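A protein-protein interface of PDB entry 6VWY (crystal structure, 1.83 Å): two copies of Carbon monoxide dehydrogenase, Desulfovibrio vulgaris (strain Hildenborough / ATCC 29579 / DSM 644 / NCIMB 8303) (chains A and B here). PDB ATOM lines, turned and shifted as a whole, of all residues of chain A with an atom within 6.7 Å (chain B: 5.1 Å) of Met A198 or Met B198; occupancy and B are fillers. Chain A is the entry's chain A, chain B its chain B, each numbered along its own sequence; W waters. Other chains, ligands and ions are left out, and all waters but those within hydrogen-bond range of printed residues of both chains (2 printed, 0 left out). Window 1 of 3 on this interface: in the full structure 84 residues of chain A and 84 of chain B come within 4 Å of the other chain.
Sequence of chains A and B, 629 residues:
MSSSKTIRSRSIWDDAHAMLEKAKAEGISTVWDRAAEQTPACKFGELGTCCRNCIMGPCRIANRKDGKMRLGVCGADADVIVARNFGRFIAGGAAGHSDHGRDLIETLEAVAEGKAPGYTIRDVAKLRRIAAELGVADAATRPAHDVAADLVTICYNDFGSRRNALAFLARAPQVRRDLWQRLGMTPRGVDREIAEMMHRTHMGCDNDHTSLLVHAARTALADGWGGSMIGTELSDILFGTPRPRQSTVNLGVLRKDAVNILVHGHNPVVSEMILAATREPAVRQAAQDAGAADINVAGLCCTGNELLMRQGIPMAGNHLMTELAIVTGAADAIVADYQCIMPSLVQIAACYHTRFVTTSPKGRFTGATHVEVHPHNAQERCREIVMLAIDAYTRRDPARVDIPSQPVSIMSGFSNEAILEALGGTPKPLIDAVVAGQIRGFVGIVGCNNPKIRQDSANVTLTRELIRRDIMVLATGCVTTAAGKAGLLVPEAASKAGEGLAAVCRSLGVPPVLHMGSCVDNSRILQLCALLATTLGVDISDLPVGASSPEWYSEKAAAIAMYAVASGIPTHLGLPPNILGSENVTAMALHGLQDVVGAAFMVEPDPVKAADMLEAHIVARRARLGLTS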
ATOM      1  N   GLY A  87       1.263  22.782  30.205  1.00  0.00           N
ATOM      2  CA  GLY A  87       1.308  23.694  29.082  1.00  0.00           C
ATOM      3  C   GLY A  87       0.043  24.525  28.975  1.00  0.00           C
ATOM      4  O   GLY A  87       0.109  25.728  28.723  1.00  0.00           O
ATOM      5  N   ARG A  88      -1.129  23.893  29.142  1.00  0.00           N
ATOM      6  CA  ARG A  88      -2.376  24.658  29.120  1.00  0.00           C
ATOM      7  C   ARG A  88      -2.450  25.626  30.289  1.00  0.00           C
ATOM      8  O   ARG A  88      -3.028  26.711  30.159  1.00  0.00           O
ATOM      9  CB  ARG A  88      -3.596  23.729  29.136  1.00  0.00           C
ATOM     10  CG  ARG A  88      -3.748  22.931  27.851  1.00  0.00           C
ATOM     11  CD  ARG A  88      -5.195  22.509  27.558  1.00  0.00           C
ATOM     12  NE  ARG A  88      -5.307  22.124  26.148  1.00  0.00           N
ATOM     13  CZ  ARG A  88      -6.391  21.586  25.593  1.00  0.00           C
ATOM     14  NH1 ARG A  88      -7.473  21.361  26.331  1.00  0.00           N
ATOM     15  NH2 ARG A  88      -6.396  21.283  24.295  1.00  0.00           N
ATOM     16  N   PHE A  89      -1.915  25.220  31.446  1.00  0.00           N
ATOM     17  CA  PHE A  89      -1.831  26.106  32.611  1.00  0.00           C
ATOM     18  C   PHE A  89      -1.042  27.367  32.265  1.00  0.00           C
ATOM     19  O   PHE A  89      -1.497  28.492  32.503  1.00  0.00           O
ATOM     20  CB  PHE A  89      -1.183  25.320  33.768  1.00  0.00           C
ATOM     21  CG  PHE A  89      -1.383  25.923  35.139  1.00  0.00           C
ATOM     22  CD1 PHE A  89      -2.474  25.556  35.918  1.00  0.00           C
ATOM     23  CD2 PHE A  89      -0.473  26.824  35.655  1.00  0.00           C
ATOM     24  CE1 PHE A  89      -2.667  26.101  37.193  1.00  0.00           C
ATOM     25  CE2 PHE A  89      -0.659  27.375  36.929  1.00  0.00           C
ATOM     26  CZ  PHE A  89      -1.758  27.009  37.691  1.00  0.00           C
ATOM     27  N   ILE A  90       0.126  27.201  31.650  1.00  0.00           N
ATOM     28  CA  ILE A  90       0.931  28.362  31.265  1.00  0.00           C
ATOM     29  C   ILE A  90       0.208  29.210  30.228  1.00  0.00           C
ATOM     30  O   ILE A  90       0.251  30.449  30.270  1.00  0.00           O
ATOM     31  CB  ILE A  90       2.304  27.907  30.744  1.00  0.00           C
ATOM     32  CG1 ILE A  90       3.135  27.268  31.876  1.00  0.00           C
ATOM     33  CG2 ILE A  90       3.019  29.062  30.026  1.00  0.00           C
ATOM     34  CD1 ILE A  90       3.603  28.214  32.939  1.00  0.00           C
ATOM     35  N   ALA A  91      -0.443  28.561  29.262  1.00  0.00           N
ATOM     36  CA  ALA A  91      -1.128  29.304  28.213  1.00  0.00           C
ATOM     37  C   ALA A  91      -2.214  30.185  28.800  1.00  0.00           C
ATOM     38  O   ALA A  91      -2.420  31.313  28.341  1.00  0.00           O
ATOM     39  CB  ALA A  91      -1.728  28.348  27.179  1.00  0.00           C
ATOM     40  N   GLY A  92      -2.922  29.683  29.814  1.00  0.00           N
ATOM     41  CA  GLY A  92      -3.952  30.492  30.451  1.00  0.00           C
ATOM     42  C   GLY A  92      -3.376  31.727  31.122  1.00  0.00           C
ATOM     43  O   GLY A  92      -3.960  32.815  31.055  1.00  0.00           O
ATOM     44  N   GLY A  93      -2.214  31.574  31.760  1.00  0.00           N
ATOM     45  CA  GLY A  93      -1.531  32.723  32.327  1.00  0.00           C
ATOM     46  C   GLY A  93      -1.053  33.698  31.272  1.00  0.00           C
ATOM     47  O   GLY A  93      -1.267  34.907  31.386  1.00  0.00           O
ATOM     48  N   ALA A  95      -2.276  34.113  28.362  1.00  0.00           N
ATOM     49  CA  ALA A  95      -3.456  34.739  27.765  1.00  0.00           C
ATOM     50  C   ALA A  95      -4.012  35.849  28.649  1.00  0.00           C
ATOM     51  O   ALA A  95      -4.517  36.861  28.144  1.00  0.00           O
ATOM     52  CB  ALA A  95      -4.531  33.686  27.498  1.00  0.00           C
ATOM     53  N   GLY A  96      -3.960  35.668  29.970  1.00  0.00           N
ATOM     54  CA  GLY A  96      -4.403  36.734  30.857  1.00  0.00           C
ATOM     55  C   GLY A  96      -3.632  38.021  30.624  1.00  0.00           C
ATOM     56  O   GLY A  96      -4.214  39.100  30.510  1.00  0.00           O
ATOM     57  N   GLU A 193       1.451  31.849  19.988  1.00  0.00           N
ATOM     58  CA  GLU A 193       2.020  30.821  20.861  1.00  0.00           C
ATOM     59  C   GLU A 193       0.949  30.194  21.732  1.00  0.00           C
ATOM     60  O   GLU A 193       0.978  28.990  21.985  1.00  0.00           O
ATOM     61  CB  GLU A 193       3.159  31.375  21.732  1.00  0.00           C
ATOM     62  CG  GLU A 193       4.254  32.160  20.978  1.00  0.00           C
ATOM     63  CD  GLU A 193       4.831  31.441  19.759  1.00  0.00           C
ATOM     64  OE1 GLU A 193       5.499  32.108  18.941  1.00  0.00           O
ATOM     65  OE2 GLU A 193       4.644  30.222  19.610  1.00  0.00           O
ATOM     66  N   ILE A 194      -0.038  30.990  22.159  1.00  0.00           N
ATOM     67  CA  ILE A 194      -1.138  30.460  22.959  1.00  0.00           C
ATOM     68  C   ILE A 194      -1.978  29.483  22.144  1.00  0.00           C
ATOM     69  O   ILE A 194      -2.323  28.386  22.615  1.00  0.00           O
ATOM     70  CB  ILE A 194      -1.993  31.620  23.501  1.00  0.00           C
ATOM     71  CG1 ILE A 194      -1.178  32.428  24.513  1.00  0.00           C
ATOM     72  CG2 ILE A 194      -3.295  31.092  24.126  1.00  0.00           C
ATOM     73  CD1 ILE A 194      -1.701  33.893  24.691  1.00  0.00           C
ATOM     74  N   ALA A 195      -2.358  29.880  20.926  1.00  0.00           N
ATOM     75  CA  ALA A 195      -3.137  28.996  20.065  1.00  0.00           C
ATOM     76  C   ALA A 195      -2.370  27.715  19.742  1.00  0.00           C
ATOM     77  O   ALA A 195      -2.940  26.616  19.759  1.00  0.00           O
ATOM     78  CB  ALA A 195      -3.515  29.719  18.771  1.00  0.00           C
ATOM     79  N   GLU A 196      -1.082  27.836  19.431  1.00  0.00           N
ATOM     80  CA  GLU A 196      -0.311  26.627  19.148  1.00  0.00           C
ATOM     81  C   GLU A 196      -0.232  25.720  20.371  1.00  0.00           C
ATOM     82  O   GLU A 196      -0.233  24.491  20.230  1.00  0.00           O
ATOM     83  CB  GLU A 196       1.100  26.961  18.666  1.00  0.00           C
ATOM     84  CG  GLU A 196       1.873  25.686  18.319  1.00  0.00           C
ATOM     85  CD  GLU A 196       3.259  25.942  17.792  1.00  0.00           C
ATOM     86  OE1 GLU A 196       4.214  25.331  18.315  1.00  0.00           O
ATOM     87  OE2 GLU A 196       3.399  26.749  16.860  1.00  0.00           O
ATOM     88  N   MET A 197      -0.188  26.291  21.582  1.00  0.00           N
ATOM     89  CA  MET A 197      -0.200  25.430  22.757  1.00  0.00           C
ATOM     90  C   MET A 197      -1.503  24.656  22.851  1.00  0.00           C
ATOM     91  O   MET A 197      -1.510  23.463  23.200  1.00  0.00           O
ATOM     92  CB  MET A 197       0.031  26.228  24.047  1.00  0.00           C
ATOM     93  CG  MET A 197       0.005  25.332  25.285  1.00  0.00           C
ATOM     94  SD  MET A 197       1.344  24.091  25.361  1.00  0.00           S
ATOM     95  CE  MET A 197       2.667  25.098  25.931  1.00  0.00           C
ATOM     96  N   MET A 198      -2.628  25.323  22.596  1.00  0.00           N
ATOM     97  CA  MET A 198      -3.900  24.620  22.661  1.00  0.00           C
ATOM     98  C   MET A 198      -3.974  23.529  21.595  1.00  0.00           C
ATOM     99  O   MET A 198      -4.538  22.456  21.838  1.00  0.00           O
ATOM    100  CB  MET A 198      -5.056  25.619  22.533  1.00  0.00           C
ATOM    101  CG  MET A 198      -5.098  26.611  23.686  1.00  0.00           C
ATOM    102  SD  MET A 198      -5.171  25.770  25.273  1.00  0.00           S
ATOM    103  CE  MET A 198      -6.807  25.029  25.216  1.00  0.00           C
ATOM    104  N   HIS A 199      -3.394  23.779  20.414  1.00  0.00           N
ATOM    105  CA  HIS A 199      -3.304  22.736  19.387  1.00  0.00           C
ATOM    106  C   HIS A 199      -2.439  21.571  19.853  1.00  0.00           C
ATOM    107  O   HIS A 199      -2.842  20.403  19.760  1.00  0.00           O
ATOM    108  CB  HIS A 199      -2.732  23.318  18.098  1.00  0.00           C
ATOM    109  CG  HIS A 199      -2.507  22.293  17.025  1.00  0.00           C
ATOM    110  ND1 HIS A 199      -1.563  22.453  16.036  1.00  0.00           N
ATOM    111  CD2 HIS A 199      -3.084  21.086  16.803  1.00  0.00           C
ATOM    112  CE1 HIS A 199      -1.589  21.406  15.228  1.00  0.00           C
ATOM    113  NE2 HIS A 199      -2.493  20.554  15.679  1.00  0.00           N
ATOM    114  N   ARG A 200      -1.230  21.873  20.340  1.00  0.00           N
ATOM    115  CA  ARG A 200      -0.323  20.829  20.801  1.00  0.00           C
ATOM    116  C   ARG A 200      -0.966  19.941  21.852  1.00  0.00           C
ATOM    117  O   ARG A 200      -0.681  18.739  21.907  1.00  0.00           O
ATOM    118  CB  ARG A 200       0.962  21.442  21.380  1.00  0.00           C
ATOM    119  CG  ARG A 200       1.962  21.885  20.315  1.00  0.00           C
ATOM    120  CD  ARG A 200       3.232  22.444  20.945  1.00  0.00           C
ATOM    121  NE  ARG A 200       4.066  23.045  19.910  1.00  0.00           N
ATOM    122  CZ  ARG A 200       5.061  22.420  19.294  1.00  0.00           C
ATOM    123  NH1 ARG A 200       5.759  23.048  18.355  1.00  0.00           N
ATOM    124  NH2 ARG A 200       5.373  21.174  19.635  1.00  0.00           N
ATOM    125  N   THR A 201      -1.842  20.494  22.685  1.00  0.00           N
ATOM    126  CA  THR A 201      -2.353  19.715  23.802  1.00  0.00           C
ATOM    127  C   THR A 201      -3.648  18.976  23.483  1.00  0.00           C
ATOM    128  O   THR A 201      -4.146  18.251  24.350  1.00  0.00           O
ATOM    129  CB  THR A 201      -2.514  20.620  25.028  1.00  0.00           C
ATOM    130  OG1 THR A 201      -3.255  21.795  24.659  1.00  0.00           O
ATOM    131  CG2 THR A 201      -1.132  21.056  25.527  1.00  0.00           C
ATOM    132  N   HIS A 202      -4.194  19.138  22.270  1.00  0.00           N
ATOM    133  CA  HIS A 202      -5.278  18.289  21.778  1.00  0.00           C
ATOM    134  C   HIS A 202      -4.802  16.841  21.718  1.00  0.00           C
ATOM    135  O   HIS A 202      -3.613  16.571  21.516  1.00  0.00           O
ATOM    136  CB  HIS A 202      -5.705  18.763  20.374  1.00  0.00           C
ATOM    137  CG  HIS A 202      -6.965  18.130  19.846  1.00  0.00           C
ATOM    138  ND1 HIS A 202      -7.029  16.822  19.413  1.00  0.00           N
ATOM    139  CD2 HIS A 202      -8.202  18.647  19.651  1.00  0.00           C
ATOM    140  CE1 HIS A 202      -8.255  16.555  18.992  1.00  0.00           C
ATOM    141  NE2 HIS A 202      -8.987  17.649  19.128  1.00  0.00           N
ATOM    142  N   MET A 203      -5.739  15.896  21.865  1.00  0.00           N
ATOM    143  CA  MET A 203      -5.375  14.481  21.750  1.00  0.00           C
ATOM    144  C   MET A 203      -4.608  14.249  20.462  1.00  0.00           C
ATOM    145  O   MET A 203      -4.967  14.769  19.401  1.00  0.00           O
ATOM    146  CB  MET A 203      -6.610  13.568  21.760  1.00  0.00           C
ATOM    147  CG  MET A 203      -6.317  12.065  21.868  1.00  0.00           C
ATOM    148  SD  MET A 203      -5.643  11.229  20.376  1.00  0.00           S
ATOM    149  CE  MET A 203      -7.052  10.233  19.893  1.00  0.00           C
ATOM    150  N   CYS A 205      -1.707  15.142  19.272  1.00  0.00           N
ATOM    151  CA  CYS A 205      -0.835  16.114  18.635  1.00  0.00           C
ATOM    152  C   CYS A 205       0.530  15.998  19.290  1.00  0.00           C
ATOM    153  O   CYS A 205       1.290  15.056  18.972  1.00  0.00           O
ATOM    154  CB  CYS A 205      -1.417  17.530  18.702  1.00  0.00           C
ATOM    155  SG  CYS A 205      -0.456  18.676  17.629  1.00  0.00           S
ATOM    156  N   HIS A 215       7.734  24.305  24.280  1.00  0.00           N
ATOM    157  CA  HIS A 215       6.748  25.261  23.779  1.00  0.00           C
ATOM    158  C   HIS A 215       6.105  26.044  24.915  1.00  0.00           C
ATOM    159  O   HIS A 215       5.716  27.197  24.719  1.00  0.00           O
ATOM    160  CB  HIS A 215       5.650  24.604  22.942  1.00  0.00           C
ATOM    161  CG  HIS A 215       4.723  25.621  22.351  1.00  0.00           C
ATOM    162  ND1 HIS A 215       5.160  26.585  21.470  1.00  0.00           N
ATOM    163  CD2 HIS A 215       3.425  25.911  22.613  1.00  0.00           C
ATOM    164  CE1 HIS A 215       4.158  27.403  21.180  1.00  0.00           C
ATOM    165  NE2 HIS A 215       3.094  27.013  21.860  1.00  0.00           N
ATOM    166  N   GLU A 555      -2.450  30.950  37.251  1.00  0.00           N
ATOM    167  CA  GLU A 555      -1.772  30.617  36.001  1.00  0.00           C
ATOM    168  C   GLU A 555      -0.866  31.761  35.554  1.00  0.00           C
ATOM    169  O   GLU A 555       0.206  31.526  34.990  1.00  0.00           O
ATOM    170  CB  GLU A 555      -2.812  30.290  34.910  1.00  0.00           C
ATOM    171  CG  GLU A 555      -3.567  28.974  35.155  1.00  0.00           C
ATOM    172  CD  GLU A 555      -4.725  28.720  34.171  1.00  0.00           C
ATOM    173  OE1 GLU A 555      -5.401  29.685  33.736  1.00  0.00           O
ATOM    174  OE2 GLU A 555      -4.974  27.535  33.843  1.00  0.00           O
ATOM    175  N   ARG B  88     -12.774  26.054  27.392  1.00  0.00           N
ATOM    176  CA  ARG B  88     -11.428  25.610  27.042  1.00  0.00           C
ATOM    177  C   ARG B  88     -11.476  24.391  26.133  1.00  0.00           C
ATOM    178  O   ARG B  88     -10.623  24.245  25.261  1.00  0.00           O
ATOM    179  CB  ARG B  88     -10.603  25.303  28.293  1.00  0.00           C
ATOM    180  CG  ARG B  88     -10.347  26.547  29.150  1.00  0.00           C
ATOM    181  CD  ARG B  88      -9.132  26.391  30.078  1.00  0.00           C
ATOM    182  NE  ARG B  88      -8.628  27.703  30.481  1.00  0.00           N
ATOM    183  CZ  ARG B  88      -7.645  27.888  31.360  1.00  0.00           C
ATOM    184  NH1 ARG B  88      -7.077  26.836  31.925  1.00  0.00           N
ATOM    185  NH2 ARG B  88      -7.245  29.120  31.681  1.00  0.00           N
ATOM    186  N   ALA B  91     -12.041  25.728  22.774  1.00  0.00           N
ATOM    187  CA  ALA B  91     -10.850  26.440  22.315  1.00  0.00           C
ATOM    188  C   ALA B  91      -9.781  25.473  21.820  1.00  0.00           C
ATOM    189  O   ALA B  91      -9.069  25.766  20.851  1.00  0.00           O
ATOM    190  CB  ALA B  91     -10.280  27.321  23.439  1.00  0.00           C
ATOM    191  N   GLY B  92      -9.630  24.325  22.486  1.00  0.00           N
ATOM    192  CA  GLY B  92      -8.664  23.347  22.019  1.00  0.00           C
ATOM    193  C   GLY B  92      -9.037  22.781  20.660  1.00  0.00           C
ATOM    194  O   GLY B  92      -8.163  22.486  19.836  1.00  0.00           O
ATOM    195  N   ALA B  95      -8.419  25.517  18.121  1.00  0.00           N
ATOM    196  CA  ALA B  95      -6.978  25.656  17.934  1.00  0.00           C
ATOM    197  C   ALA B  95      -6.422  24.568  17.031  1.00  0.00           C
ATOM    198  O   ALA B  95      -5.520  24.824  16.225  1.00  0.00           O
ATOM    199  CB  ALA B  95      -6.271  25.645  19.292  1.00  0.00           C
ATOM    200  N   ILE B 194      -9.392  32.334  20.455  1.00  0.00           N
ATOM    201  CA  ILE B 194      -8.803  31.290  21.297  1.00  0.00           C
ATOM    202  C   ILE B 194      -8.095  31.905  22.492  1.00  0.00           C
ATOM    203  O   ILE B 194      -8.233  31.437  23.631  1.00  0.00           O
ATOM    204  CB  ILE B 194      -7.837  30.423  20.464  1.00  0.00           C
ATOM    205  CG1 ILE B 194      -8.615  29.632  19.419  1.00  0.00           C
ATOM    206  CG2 ILE B 194      -7.020  29.453  21.356  1.00  0.00           C
ATOM    207  CD1 ILE B 194      -7.749  29.116  18.254  1.00  0.00           C
ATOM    208  N   ALA B 195      -7.269  32.925  22.242  1.00  0.00           N
ATOM    209  CA  ALA B 195      -6.549  33.569  23.336  1.00  0.00           C
ATOM    210  C   ALA B 195      -7.513  34.218  24.316  1.00  0.00           C
ATOM    211  O   ALA B 195      -7.310  34.151  25.533  1.00  0.00           O
ATOM    212  CB  ALA B 195      -5.568  34.614  22.792  1.00  0.00           C
ATOM    213  N   GLU B 196      -8.568  34.854  23.805  1.00  0.00           N
ATOM    214  CA  GLU B 196      -9.532  35.471  24.710  1.00  0.00           C
ATOM    215  C   GLU B 196     -10.262  34.422  25.540  1.00  0.00           C
ATOM    216  O   GLU B 196     -10.582  34.666  26.709  1.00  0.00           O
ATOM    217  CB  GLU B 196     -10.540  36.319  23.936  1.00  0.00           C
ATOM    218  CG  GLU B 196     -11.450  37.082  24.907  1.00  0.00           C
ATOM    219  CD  GLU B 196     -12.475  37.972  24.230  1.00  0.00           C
ATOM    220  OE1 GLU B 196     -13.682  37.755  24.456  1.00  0.00           O
ATOM    221  OE2 GLU B 196     -12.074  38.889  23.495  1.00  0.00           O
ATOM    222  N   MET B 197     -10.531  33.249  24.964  1.00  0.00           N
ATOM    223  CA  MET B 197     -11.154  32.197  25.757  1.00  0.00           C
ATOM    224  C   MET B 197     -10.243  31.757  26.897  1.00  0.00           C
ATOM    225  O   MET B 197     -10.712  31.527  28.015  1.00  0.00           O
ATOM    226  CB  MET B 197     -11.530  30.997  24.887  1.00  0.00           C
ATOM    227  CG  MET B 197     -12.146  29.850  25.710  1.00  0.00           C
ATOM    228  SD  MET B 197     -13.748  30.311  26.471  1.00  0.00           S
ATOM    229  CE  MET B 197     -14.800  30.024  25.070  1.00  0.00           C
ATOM    230  N   MET B 198      -8.937  31.602  26.629  1.00  0.00           N
ATOM    231  CA  MET B 198      -8.034  31.213  27.707  1.00  0.00           C
ATOM    232  C   MET B 198      -7.947  32.298  28.778  1.00  0.00           C
ATOM    233  O   MET B 198      -7.783  31.988  29.965  1.00  0.00           O
ATOM    234  CB  MET B 198      -6.651  30.875  27.143  1.00  0.00           C
ATOM    235  CG  MET B 198      -6.670  29.675  26.190  1.00  0.00           C
ATOM    236  SD  MET B 198      -7.341  28.226  27.039  1.00  0.00           S
ATOM    237  CE  MET B 198      -5.980  27.815  28.146  1.00  0.00           C
ATOM    238  N   HIS B 199      -8.056  33.572  28.379  1.00  0.00           N
ATOM    239  CA  HIS B 199      -8.083  34.655  29.361  1.00  0.00           C
ATOM    240  C   HIS B 199      -9.362  34.610  30.182  1.00  0.00           C
ATOM    241  O   HIS B 199      -9.328  34.733  31.415  1.00  0.00           O
ATOM    242  CB  HIS B 199      -7.952  36.008  28.667  1.00  0.00           C
ATOM    243  CG  HIS B 199      -8.170  37.176  29.584  1.00  0.00           C
ATOM    244  ND1 HIS B 199      -8.709  38.368  29.152  1.00  0.00           N
ATOM    245  CD2 HIS B 199      -7.942  37.326  30.913  1.00  0.00           C
ATOM    246  CE1 HIS B 199      -8.784  39.213  30.166  1.00  0.00           C
ATOM    247  NE2 HIS B 199      -8.331  38.601  31.250  1.00  0.00           N
ATOM    248  N   ARG B 200     -10.506  34.425  29.507  1.00  0.00           N
ATOM    249  CA  ARG B 200     -11.793  34.434  30.193  1.00  0.00           C
ATOM    250  C   ARG B 200     -11.891  33.330  31.230  1.00  0.00           C
ATOM    251  O   ARG B 200     -12.584  33.491  32.237  1.00  0.00           O
ATOM    252  CB  ARG B 200     -12.931  34.283  29.178  1.00  0.00           C
ATOM    253  CG  ARG B 200     -13.291  35.564  28.449  1.00  0.00           C
ATOM    254  CD  ARG B 200     -14.416  35.280  27.418  1.00  0.00           C
ATOM    255  NE  ARG B 200     -14.731  36.491  26.666  1.00  0.00           N
ATOM    256  CZ  ARG B 200     -15.675  37.360  27.006  1.00  0.00           C
ATOM    257  NH1 ARG B 200     -15.879  38.436  26.255  1.00  0.00           N
ATOM    258  NH2 ARG B 200     -16.422  37.154  28.086  1.00  0.00           N
ATOM    259  N   THR B 201     -11.217  32.204  31.005  1.00  0.00           N
ATOM    260  CA  THR B 201     -11.339  31.067  31.904  1.00  0.00           C
ATOM    261  C   THR B 201     -10.262  31.032  32.990  1.00  0.00           C
ATOM    262  O   THR B 201     -10.274  30.121  33.828  1.00  0.00           O
ATOM    263  CB  THR B 201     -11.331  29.780  31.082  1.00  0.00           C
ATOM    264  OG1 THR B 201     -10.218  29.801  30.183  1.00  0.00           O
ATOM    265  CG2 THR B 201     -12.630  29.701  30.243  1.00  0.00           C
ATOM    266  N   HIS B 202      -9.344  31.994  33.002  1.00  0.00           N
ATOM    267  CA  HIS B 202      -8.479  32.205  34.160  1.00  0.00           C
ATOM    268  C   HIS B 202      -9.333  32.516  35.387  1.00  0.00           C
ATOM    269  O   HIS B 202     -10.422  33.072  35.274  1.00  0.00           O
ATOM    270  CB  HIS B 202      -7.508  33.361  33.878  1.00  0.00           C
ATOM    271  CG  HIS B 202      -6.394  33.499  34.877  1.00  0.00           C
ATOM    272  ND1 HIS B 202      -6.564  34.097  36.107  1.00  0.00           N
ATOM    273  CD2 HIS B 202      -5.086  33.141  34.812  1.00  0.00           C
ATOM    274  CE1 HIS B 202      -5.414  34.098  36.762  1.00  0.00           C
ATOM    275  NE2 HIS B 202      -4.501  33.520  35.998  1.00  0.00           N
HETATM  276  O   HOH W   1      -5.274  24.840  34.066  1.00  0.00           O
HETATM  277  O   HOH W   2      -6.156  30.815  36.535  1.00  0.00           O
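Of the 13 printed residues of chain B, 7 touch a printed residue of chain A. Among the printed residues, 18 pairs touch across the chains. Among the printed residues, Asp or Glu carboxylates within 4 Å of a Lys or Arg side-chain nitrogen of the other chain: Glu A555 with Arg B88 (2.8 Å).
NH2 of Arg A88 touches CA of Gly B92, 3.8 Å away. Arg A88 touches Met B198. Gly A92 touches Arg B88. Ala B195 touches Ala A95 (O to CB, 3.4 Å). CB of Met B198 touches CB of Ala A95, 3.5 Å away. Ala A95 touches His B199. CA of Gly A96 touches CD2 of His B199 (3.6 Å). Met A198 touches Gly B92. His A199 touches Ala B95. His B202 touches Glu A555 (NE2 to N, 3.5 Å).
Water W1 bridges the side-chain carboxylate (OE2) of Glu A555 (2.7 Å) and the guanidinium group (NH1) of Arg B88 (3.4 Å). Water W2 lies within hydrogen-bond range of the side-chain carboxylate of Glu A555 (3.1 Å) and a ring nitrogen (NE2) of His B202 (3.2 Å).
Printed residues of chain B within 4 Å of Met A198: Arg B88 (3.9 Å), Gly B92 (3.99 Å), Ala B95 (3.5 Å) and Met B198 (3.6 Å). Of chain A, only Arg A88, Gly A92, Ala A95 and Met A198 come within 4 Å of Met B198. Printed residues of chain A within 4 Å of His B202: Gly A92 and Glu A555. Printed residues of chain A within 4 Å of Ala B195: Ala A95 (3.4 Å). Thr B201 touches none of the printed residues of chain A. Gly A93 touches none of the printed residues of chain B. The nearest residue of chain A that does not touch Met B198 is Ile A194 (4.2 Å).
The guanidinium group (NH2) of Arg B88 is in salt-bridge range of the side-chain carboxylate (OE1) of Glu A555 (2.8 Å). The side-chain sulfur of Met B198 lies close to the side-chain sulfur of Met A198.
The guanidinium group (NH2) of Arg A88 lies within hydrogen-bond range of the backbone carbonyl oxygen (O) of Met A198. The side-chain hydroxyl of Thr A201 sits at hydrogen-bond distance from the backbone carbonyl oxygen of Met A198, at 3.2 Å. The side-chain sulfur (SG) of Cys A205 sits at hydrogen-bond distance from a ring nitrogen (NE2) of His A199, 3.4 Å away. The backbone carbonyl oxygen (O) of Met B198 sits at hydrogen-bond distance from the guanidinium group (NH2) of Arg B88 (3.4 Å). The guanidinium group (NE) of Arg B88 sits at hydrogen-bond distance from the side-chain hydroxyl (OG1) of Thr B201, at 2.6 Å. The side-chain hydroxyl (OG1) of Thr B201 lies within hydrogen-bond range of the backbone carbonyl oxygen (O) of Met B198.
Arg A88 touches Gly B92, and with the chains exchanged Gly A92 touches Arg B88. Gly A92 touches Met B198, and with the chains exchanged Met A198 touches Gly B92. Ala A95 touches Ala B195, and with the chains exchanged Ala A195 touches Ala B95. Ala A95 touches His B199, and with the chains exchanged His A199 touches Ala B95.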
